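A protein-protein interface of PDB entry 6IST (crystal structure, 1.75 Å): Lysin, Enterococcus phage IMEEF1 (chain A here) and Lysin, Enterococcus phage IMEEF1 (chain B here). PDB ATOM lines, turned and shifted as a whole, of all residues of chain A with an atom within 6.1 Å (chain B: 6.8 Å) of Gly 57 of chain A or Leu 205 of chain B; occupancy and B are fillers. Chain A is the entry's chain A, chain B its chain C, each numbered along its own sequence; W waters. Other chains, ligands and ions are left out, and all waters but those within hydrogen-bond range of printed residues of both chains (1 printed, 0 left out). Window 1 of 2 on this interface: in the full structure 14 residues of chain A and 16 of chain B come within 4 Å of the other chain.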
ATOM      1  N   TYR A  51       9.215  32.626 -33.390  1.00  0.00           N
ATOM      2  CA  TYR A  51       9.207  33.359 -32.121  1.00  0.00           C
ATOM      3  C   TYR A  51      10.344  34.347 -32.063  1.00  0.00           C
ATOM      4  O   TYR A  51      11.498  33.970 -32.256  1.00  0.00           O
ATOM      5  CB  TYR A  51       9.388  32.369 -30.943  1.00  0.00           C
ATOM      6  CG  TYR A  51       8.252  31.346 -30.764  1.00  0.00           C
ATOM      7  CD1 TYR A  51       8.246  30.143 -31.482  1.00  0.00           C
ATOM      8  CD2 TYR A  51       7.222  31.588 -29.858  1.00  0.00           C
ATOM      9  CE1 TYR A  51       7.266  29.187 -31.299  1.00  0.00           C
ATOM     10  CE2 TYR A  51       6.175  30.669 -29.704  1.00  0.00           C
ATOM     11  CZ  TYR A  51       6.213  29.468 -30.418  1.00  0.00           C
ATOM     12  OH  TYR A  51       5.210  28.560 -30.263  1.00  0.00           O
ATOM     13  N   ASN A  55       9.687  36.795 -26.822  1.00  0.00           N
ATOM     14  CA  ASN A  55       8.325  36.270 -26.708  1.00  0.00           C
ATOM     15  C   ASN A  55       8.180  35.418 -25.458  1.00  0.00           C
ATOM     16  O   ASN A  55       9.016  34.540 -25.225  1.00  0.00           O
ATOM     17  CB  ASN A  55       7.982  35.420 -27.902  1.00  0.00           C
ATOM     18  CG  ASN A  55       6.576  34.886 -27.825  1.00  0.00           C
ATOM     19  OD1 ASN A  55       6.369  33.829 -27.290  1.00  0.00           O
ATOM     20  ND2 ASN A  55       5.619  35.643 -28.255  1.00  0.00           N
ATOM     21  N   PHE A  56       7.165  35.694 -24.640  1.00  0.00           N
ATOM     22  CA  PHE A  56       7.003  34.905 -23.400  1.00  0.00           C
ATOM     23  C   PHE A  56       6.655  33.425 -23.611  1.00  0.00           C
ATOM     24  O   PHE A  56       7.024  32.593 -22.795  1.00  0.00           O
ATOM     25  CB  PHE A  56       5.940  35.510 -22.463  1.00  0.00           C
ATOM     26  CG  PHE A  56       6.264  36.891 -21.876  1.00  0.00           C
ATOM     27  CD1 PHE A  56       7.487  37.503 -22.004  1.00  0.00           C
ATOM     28  CD2 PHE A  56       5.280  37.553 -21.117  1.00  0.00           C
ATOM     29  CE1 PHE A  56       7.737  38.743 -21.421  1.00  0.00           C
ATOM     30  CE2 PHE A  56       5.539  38.792 -20.528  1.00  0.00           C
ATOM     31  CZ  PHE A  56       6.747  39.389 -20.693  1.00  0.00           C
ATOM     32  N   GLY A  57       5.991  33.063 -24.693  1.00  0.00           N
ATOM     33  CA  GLY A  57       5.831  31.641 -25.000  1.00  0.00           C
ATOM     34  C   GLY A  57       7.176  30.946 -25.224  1.00  0.00           C
ATOM     35  O   GLY A  57       7.457  29.881 -24.672  1.00  0.00           O
ATOM     36  N   LEU A  58       8.020  31.560 -26.039  1.00  0.00           N
ATOM     37  CA  LEU A  58       9.400  31.118 -26.201  1.00  0.00           C
ATOM     38  C   LEU A  58      10.119  31.024 -24.852  1.00  0.00           C
ATOM     39  O   LEU A  58      10.741  29.989 -24.522  1.00  0.00           O
ATOM     40  CB  LEU A  58      10.171  32.025 -27.129  1.00  0.00           C
ATOM     41  CG  LEU A  58      11.638  31.586 -27.356  1.00  0.00           C
ATOM     42  CD1 LEU A  58      11.723  30.133 -27.852  1.00  0.00           C
ATOM     43  CD2 LEU A  58      12.356  32.551 -28.329  1.00  0.00           C
ATOM     44  N   LYS A  59      10.037  32.081 -24.050  1.00  0.00           N
ATOM     45  CA  LYS A  59      10.735  32.065 -22.765  1.00  0.00           C
ATOM     46  C   LYS A  59      10.291  30.925 -21.866  1.00  0.00           C
ATOM     47  O   LYS A  59      11.142  30.203 -21.225  1.00  0.00           O
ATOM     48  CB  LYS A  59      10.590  33.390 -22.055  1.00  0.00           C
ATOM     49  CG  LYS A  59      11.300  34.560 -22.702  1.00  0.00           C
ATOM     50  CD  LYS A  59      12.803  34.495 -22.442  1.00  0.00           C
ATOM     51  CE  LYS A  59      13.440  35.800 -22.909  1.00  0.00           C
ATOM     52  NZ  LYS A  59      14.916  35.647 -22.937  1.00  0.00           N
ATOM     53  N   MET A  60       8.985  30.660 -21.842  1.00  0.00           N
ATOM     54  CA  MET A  60       8.491  29.520 -21.061  1.00  0.00           C
ATOM     55  C   MET A  60       8.954  28.128 -21.638  1.00  0.00           C
ATOM     56  O   MET A  60       9.435  27.268 -20.903  1.00  0.00           O
ATOM     57  CB  MET A  60       6.937  29.628 -20.933  1.00  0.00           C
ATOM     58  CG  MET A  60       6.453  30.686 -19.924  1.00  0.00           C
ATOM     59  SD  MET A  60       4.650  30.664 -19.796  1.00  0.00           S
ATOM     60  CE  MET A  60       4.230  31.267 -21.413  1.00  0.00           C
ATOM     61  N   MET A  61       8.976  27.956 -22.961  1.00  0.00           N
ATOM     62  CA  MET A  61       9.546  26.727 -23.538  1.00  0.00           C
ATOM     63  C   MET A  61      11.042  26.611 -23.187  1.00  0.00           C
ATOM     64  O   MET A  61      11.494  25.523 -22.787  1.00  0.00           O
ATOM     65  CB  MET A  61       9.386  26.682 -25.050  1.00  0.00           C
ATOM     66  CG  MET A  61       7.941  26.487 -25.536  1.00  0.00           C
ATOM     67  SD  MET A  61       7.774  26.033 -27.364  1.00  0.00           S
ATOM     68  CE  MET A  61       8.082  27.633 -28.041  1.00  0.00           C
ATOM     69  N   GLU A  62      11.798  27.720 -23.230  1.00  0.00           N
ATOM     70  CA  GLU A  62      13.264  27.599 -23.008  1.00  0.00           C
ATOM     71  C   GLU A  62      13.555  27.234 -21.551  1.00  0.00           C
ATOM     72  O   GLU A  62      14.506  26.476 -21.254  1.00  0.00           O
ATOM     73  CB  GLU A  62      13.993  28.864 -23.442  1.00  0.00           C
ATOM     74  CG  GLU A  62      13.950  29.060 -24.975  1.00  0.00           C
ATOM     75  CD  GLU A  62      14.665  30.323 -25.479  1.00  0.00           C
ATOM     76  OE1 GLU A  62      14.716  31.334 -24.734  1.00  0.00           O
ATOM     77  OE2 GLU A  62      15.196  30.325 -26.628  1.00  0.00           O
ATOM     78  N   MET B 168       0.396  19.506 -22.012  1.00  0.00           N
ATOM     79  CA  MET B 168       0.457  20.952 -21.885  1.00  0.00           C
ATOM     80  C   MET B 168      -0.954  21.366 -21.454  1.00  0.00           C
ATOM     81  O   MET B 168      -1.897  21.036 -22.166  1.00  0.00           O
ATOM     82  CB  MET B 168       0.746  21.559 -23.253  1.00  0.00           C
ATOM     83  CG  MET B 168       1.684  22.713 -23.335  1.00  0.00           C
ATOM     84  SD  MET B 168       1.825  23.244 -25.070  1.00  0.00           S
ATOM     85  CE  MET B 168       3.165  22.180 -25.520  1.00  0.00           C
ATOM     86  N   PHE B 184       1.018  26.707 -15.468  1.00  0.00           N
ATOM     87  CA  PHE B 184       1.137  26.076 -16.802  1.00  0.00           C
ATOM     88  C   PHE B 184       1.995  24.866 -16.712  1.00  0.00           C
ATOM     89  O   PHE B 184       3.103  24.939 -16.247  1.00  0.00           O
ATOM     90  CB  PHE B 184       1.680  27.104 -17.734  1.00  0.00           C
ATOM     91  CG  PHE B 184       1.843  26.684 -19.175  1.00  0.00           C
ATOM     92  CD1 PHE B 184       0.875  26.004 -19.844  1.00  0.00           C
ATOM     93  CD2 PHE B 184       2.983  27.078 -19.856  1.00  0.00           C
ATOM     94  CE1 PHE B 184       1.054  25.663 -21.165  1.00  0.00           C
ATOM     95  CE2 PHE B 184       3.172  26.770 -21.191  1.00  0.00           C
ATOM     96  CZ  PHE B 184       2.192  26.041 -21.838  1.00  0.00           C
ATOM     97  N   ILE B 186       4.024  22.160 -18.824  1.00  0.00           N
ATOM     98  CA  ILE B 186       4.662  21.982 -20.109  1.00  0.00           C
ATOM     99  C   ILE B 186       5.993  21.268 -19.900  1.00  0.00           C
ATOM    100  O   ILE B 186       6.712  21.585 -18.968  1.00  0.00           O
ATOM    101  CB  ILE B 186       4.912  23.348 -20.809  1.00  0.00           C
ATOM    102  CG1 ILE B 186       5.638  23.165 -22.141  1.00  0.00           C
ATOM    103  CG2 ILE B 186       5.656  24.314 -19.910  1.00  0.00           C
ATOM    104  CD1 ILE B 186       5.611  24.338 -23.078  1.00  0.00           C
ATOM    105  N   THR B 197      -0.357  38.423 -19.609  1.00  0.00           N
ATOM    106  CA  THR B 197       0.351  38.208 -20.911  1.00  0.00           C
ATOM    107  C   THR B 197       1.026  36.868 -20.923  1.00  0.00           C
ATOM    108  O   THR B 197       1.071  36.219 -21.954  1.00  0.00           O
ATOM    109  CB  THR B 197       1.391  39.294 -21.178  1.00  0.00           C
ATOM    110  OG1 THR B 197       0.734  40.577 -21.094  1.00  0.00           O
ATOM    111  CG2 THR B 197       2.043  39.116 -22.633  1.00  0.00           C
ATOM    112  N   TYR B 198       1.528  36.431 -19.763  1.00  0.00           N
ATOM    113  CA  TYR B 198       1.985  35.068 -19.637  1.00  0.00           C
ATOM    114  C   TYR B 198       0.856  34.058 -19.868  1.00  0.00           C
ATOM    115  O   TYR B 198       1.033  33.113 -20.645  1.00  0.00           O
ATOM    116  CB  TYR B 198       2.692  34.827 -18.348  1.00  0.00           C
ATOM    117  CG  TYR B 198       4.101  35.386 -18.340  1.00  0.00           C
ATOM    118  CD1 TYR B 198       5.125  34.689 -18.914  1.00  0.00           C
ATOM    119  CD2 TYR B 198       4.391  36.576 -17.678  1.00  0.00           C
ATOM    120  CE1 TYR B 198       6.433  35.208 -18.894  1.00  0.00           C
ATOM    121  CE2 TYR B 198       5.683  37.090 -17.640  1.00  0.00           C
ATOM    122  CZ  TYR B 198       6.693  36.393 -18.246  1.00  0.00           C
ATOM    123  OH  TYR B 198       7.959  36.890 -18.215  1.00  0.00           O
ATOM    124  N   ASN B 200      -1.952  34.538 -21.658  1.00  0.00           N
ATOM    125  CA  ASN B 200      -2.245  34.553 -23.076  1.00  0.00           C
ATOM    126  C   ASN B 200      -1.224  33.795 -23.943  1.00  0.00           C
ATOM    127  O   ASN B 200      -1.587  33.025 -24.878  1.00  0.00           O
ATOM    128  CB  ASN B 200      -2.392  36.020 -23.548  1.00  0.00           C
ATOM    129  CG  ASN B 200      -3.656  36.700 -22.971  1.00  0.00           C
ATOM    130  OD1 ASN B 200      -4.571  36.056 -22.437  1.00  0.00           O
ATOM    131  ND2 ASN B 200      -3.695  38.001 -23.086  1.00  0.00           N
ATOM    132  N   GLU B 201       0.035  33.992 -23.650  1.00  0.00           N
ATOM    133  CA  GLU B 201       1.040  33.226 -24.370  1.00  0.00           C
ATOM    134  C   GLU B 201       0.969  31.676 -24.107  1.00  0.00           C
ATOM    135  O   GLU B 201       1.184  30.847 -25.022  1.00  0.00           O
ATOM    136  CB  GLU B 201       2.442  33.795 -24.099  1.00  0.00           C
ATOM    137  CG  GLU B 201       2.602  35.240 -24.563  1.00  0.00           C
ATOM    138  CD  GLU B 201       2.794  35.400 -26.078  1.00  0.00           C
ATOM    139  OE1 GLU B 201       2.928  34.376 -26.806  1.00  0.00           O
ATOM    140  OE2 GLU B 201       2.775  36.563 -26.525  1.00  0.00           O
ATOM    141  N   ALA B 202       0.728  31.261 -22.864  1.00  0.00           N
ATOM    142  CA  ALA B 202       0.552  29.850 -22.571  1.00  0.00           C
ATOM    143  C   ALA B 202      -0.661  29.323 -23.288  1.00  0.00           C
ATOM    144  O   ALA B 202      -0.568  28.239 -23.883  1.00  0.00           O
ATOM    145  CB  ALA B 202       0.451  29.584 -21.080  1.00  0.00           C
ATOM    146  N   ASN B 203      -1.773  30.084 -23.341  1.00  0.00           N
ATOM    147  CA  ASN B 203      -2.913  29.611 -24.137  1.00  0.00           C
ATOM    148  C   ASN B 203      -2.618  29.504 -25.637  1.00  0.00           C
ATOM    149  O   ASN B 203      -3.182  28.624 -26.353  1.00  0.00           O
ATOM    150  CB  ASN B 203      -4.198  30.400 -23.872  1.00  0.00           C
ATOM    151  CG  ASN B 203      -4.896  29.880 -22.619  1.00  0.00           C
ATOM    152  OD1 ASN B 203      -5.147  28.663 -22.494  1.00  0.00           O
ATOM    153  ND2 ASN B 203      -5.173  30.745 -21.705  1.00  0.00           N
ATOM    154  N   ASP B 204      -1.759  30.364 -26.115  1.00  0.00           N
ATOM    155  CA  ASP B 204      -1.347  30.279 -27.523  1.00  0.00           C
ATOM    156  C   ASP B 204      -0.537  29.029 -27.771  1.00  0.00           C
ATOM    157  O   ASP B 204      -0.728  28.381 -28.799  1.00  0.00           O
ATOM    158  CB  ASP B 204      -0.572  31.504 -27.945  1.00  0.00           C
ATOM    159  CG  ASP B 204      -1.464  32.744 -28.073  1.00  0.00           C
ATOM    160  OD1 ASP B 204      -2.724  32.600 -28.119  1.00  0.00           O
ATOM    161  OD2 ASP B 204      -0.894  33.861 -28.127  1.00  0.00           O
ATOM    162  N   LEU B 205       0.362  28.680 -26.848  1.00  0.00           N
ATOM    163  CA  LEU B 205       1.086  27.420 -26.938  1.00  0.00           C
ATOM    164  C   LEU B 205       0.127  26.222 -26.976  1.00  0.00           C
ATOM    165  O   LEU B 205       0.218  25.343 -27.867  1.00  0.00           O
ATOM    166  CB  LEU B 205       2.069  27.276 -25.790  1.00  0.00           C
ATOM    167  CG  LEU B 205       3.269  28.226 -25.740  1.00  0.00           C
ATOM    168  CD1 LEU B 205       4.047  27.979 -24.475  1.00  0.00           C
ATOM    169  CD2 LEU B 205       4.142  27.960 -26.903  1.00  0.00           C
ATOM    170  N   ILE B 206      -0.822  26.212 -26.026  1.00  0.00           N
ATOM    171  CA  ILE B 206      -1.842  25.195 -25.998  1.00  0.00           C
ATOM    172  C   ILE B 206      -2.532  25.015 -27.313  1.00  0.00           C
ATOM    173  O   ILE B 206      -2.724  23.846 -27.768  1.00  0.00           O
ATOM    174  CB  ILE B 206      -2.822  25.443 -24.853  1.00  0.00           C
ATOM    175  CG1 ILE B 206      -2.070  25.135 -23.563  1.00  0.00           C
ATOM    176  CG2 ILE B 206      -4.060  24.535 -24.962  1.00  0.00           C
ATOM    177  CD1 ILE B 206      -2.811  25.585 -22.284  1.00  0.00           C
ATOM    178  N   LYS B 207      -2.918  26.129 -27.906  1.00  0.00           N
ATOM    179  CA  LYS B 207      -3.568  26.091 -29.227  1.00  0.00           C
ATOM    180  C   LYS B 207      -2.710  25.522 -30.342  1.00  0.00           C
ATOM    181  O   LYS B 207      -3.180  24.686 -31.135  1.00  0.00           O
ATOM    182  CB  LYS B 207      -4.104  27.448 -29.640  1.00  0.00           C
ATOM    183  CG  LYS B 207      -5.579  27.678 -29.333  1.00  0.00           C
ATOM    184  CD  LYS B 207      -6.053  28.947 -30.044  1.00  0.00           C
ATOM    185  CE  LYS B 207      -7.047  29.761 -29.221  1.00  0.00           C
ATOM    186  NZ  LYS B 207      -8.396  29.138 -29.245  1.00  0.00           N
ATOM    187  N   ARG B 208      -1.471  25.971 -30.423  1.00  0.00           N
ATOM    188  CA  ARG B 208      -0.557  25.524 -31.462  1.00  0.00           C
ATOM    189  C   ARG B 208      -0.180  24.040 -31.438  1.00  0.00           C
ATOM    190  O   ARG B 208      -0.021  23.379 -32.487  1.00  0.00           O
ATOM    191  CB  ARG B 208       0.761  26.302 -31.329  1.00  0.00           C
ATOM    192  CG  ARG B 208       0.685  27.710 -31.727  1.00  0.00           C
ATOM    193  CD  ARG B 208       2.031  28.386 -31.615  1.00  0.00           C
ATOM    194  NE  ARG B 208       1.734  29.788 -31.615  1.00  0.00           N
ATOM    195  CZ  ARG B 208       2.109  30.653 -30.700  1.00  0.00           C
ATOM    196  NH1 ARG B 208       2.884  30.305 -29.658  1.00  0.00           N
ATOM    197  NH2 ARG B 208       1.676  31.893 -30.804  1.00  0.00           N
ATOM    198  N   TYR B 209       0.077  23.560 -30.244  1.00  0.00           N
ATOM    199  CA  TYR B 209       0.714  22.304 -30.051  1.00  0.00           C
ATOM    200  C   TYR B 209      -0.234  21.214 -29.521  1.00  0.00           C
ATOM    201  O   TYR B 209       0.220  20.162 -29.064  1.00  0.00           O
ATOM    202  CB  TYR B 209       1.978  22.458 -29.212  1.00  0.00           C
ATOM    203  CG  TYR B 209       2.974  23.461 -29.788  1.00  0.00           C
ATOM    204  CD1 TYR B 209       3.467  23.341 -31.101  1.00  0.00           C
ATOM    205  CD2 TYR B 209       3.405  24.561 -29.052  1.00  0.00           C
ATOM    206  CE1 TYR B 209       4.358  24.249 -31.641  1.00  0.00           C
ATOM    207  CE2 TYR B 209       4.284  25.495 -29.597  1.00  0.00           C
ATOM    208  CZ  TYR B 209       4.775  25.324 -30.894  1.00  0.00           C
ATOM    209  OH  TYR B 209       5.670  26.224 -31.448  1.00  0.00           O
ATOM    210  N   GLY B 210      -1.525  21.510 -29.577  1.00  0.00           N
ATOM    211  CA  GLY B 210      -2.582  20.586 -29.194  1.00  0.00           C
ATOM    212  C   GLY B 210      -2.550  20.230 -27.733  1.00  0.00           C
ATOM    213  O   GLY B 210      -2.656  19.078 -27.378  1.00  0.00           O
ATOM    214  N   GLY B 211      -2.345  21.217 -26.880  1.00  0.00           N
ATOM    215  CA  GLY B 211      -2.493  21.015 -25.445  1.00  0.00           C
ATOM    216  C   GLY B 211      -3.953  20.831 -25.057  1.00  0.00           C
ATOM    217  O   GLY B 211      -4.822  21.001 -25.876  1.00  0.00           O
HETATM  218  O   HOH W   1       5.356  37.815 -25.196  1.00  0.00           O
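The side-chain hydroxyl (OH) of Tyr 51 of chain A lies within hydrogen-bond range of the guanidinium group (NH1) of Arg 208 of chain B, at 3.0 Å.
OH of Tyr 51 of chain A is in hydrogen-bond range of OH of Tyr 209 of chain B, at 2.7 Å.
The side-chain carboxylate of Glu 201 of chain B sits at hydrogen-bond distance from the side-chain amide nitrogen of Asn 55 of chain A, at 3.3 Å.
Leu 205 of chain B touches Tyr 51 of chain A (CD2 to OH, 3.6 Å).
Phe 56 of chain A touches Thr 197 of chain B (CD2 to CG2, 3.9 Å).
CE2 of Phe 56 of chain A touches CE2 of Tyr 198 of chain B (3.4 Å).
Glu 201 of chain B touches Phe 56 of chain A.
Glu 201 of chain B touches Gly 57 of chain A.
O of Gly 57 of chain A touches CD1 of Leu 205 of chain B, 3.9 Å away.
Met 60 of chain A touches Phe 184 of chain B.
Met 60 of chain A touches Tyr 198 of chain B.
Ala 202 of chain B touches Met 60 of chain A (N to CE, 3.8 Å).
The side-chain amide oxygen (OD1) of Asn 55 of chain A is in hydrogen-bond range of the backbone NH (N) of Gly 57 of chain A (2.7 Å).
OD1 of Asn 55 of chain A lies within hydrogen-bond range of N of Leu 58 of chain A (3.1 Å).
Gly 57 of chain A touches just these residues of chain B: Glu 201 and Leu 205.
Of the printed residues of chain B, Asn 55 of chain A touches Glu 201 (3.3 Å).
Of the printed residues of chain B, Met 60 of chain A touches Phe 184 (3.95 Å), Tyr 198 (3.8 Å) and Ala 202 (3.8 Å).
Printed residues of chain A within 4 Å of Phe 184 of chain B: Met 60 (3.95 Å).
Printed residues of chain A within 4 Å of Glu 201 of chain B: Asn 55 (3.3 Å), Phe 56 (3.95 Å) and Gly 57 (3.7 Å).
The nearest residue of chain B that does not touch Gly 57 of chain A is Ala 202 of chain B (5.5 Å).
The nearest residue of chain A that does not touch Leu 205 of chain B is Met 61 of chain A (4.1 Å).
Of the 17 printed residues of chain B, 8 touch a printed residue of chain A.
Hydrophobic or aromatic side chains of chain B within 4 Å of the printed part of chain A: Phe 184, Tyr 198, Leu 205 and Tyr 209.
Along chain B the printed residues that touch a printed residue of chain A span positions 184 to 209.
Of the 9 printed residues of chain A, 5 touch a printed residue of chain B.
Water W1 lies within hydrogen-bond range of the backbone NH of Phe 56 of chain A (2.8 Å) and the side-chain carboxylate of Glu 201 of chain B (3.2 Å).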
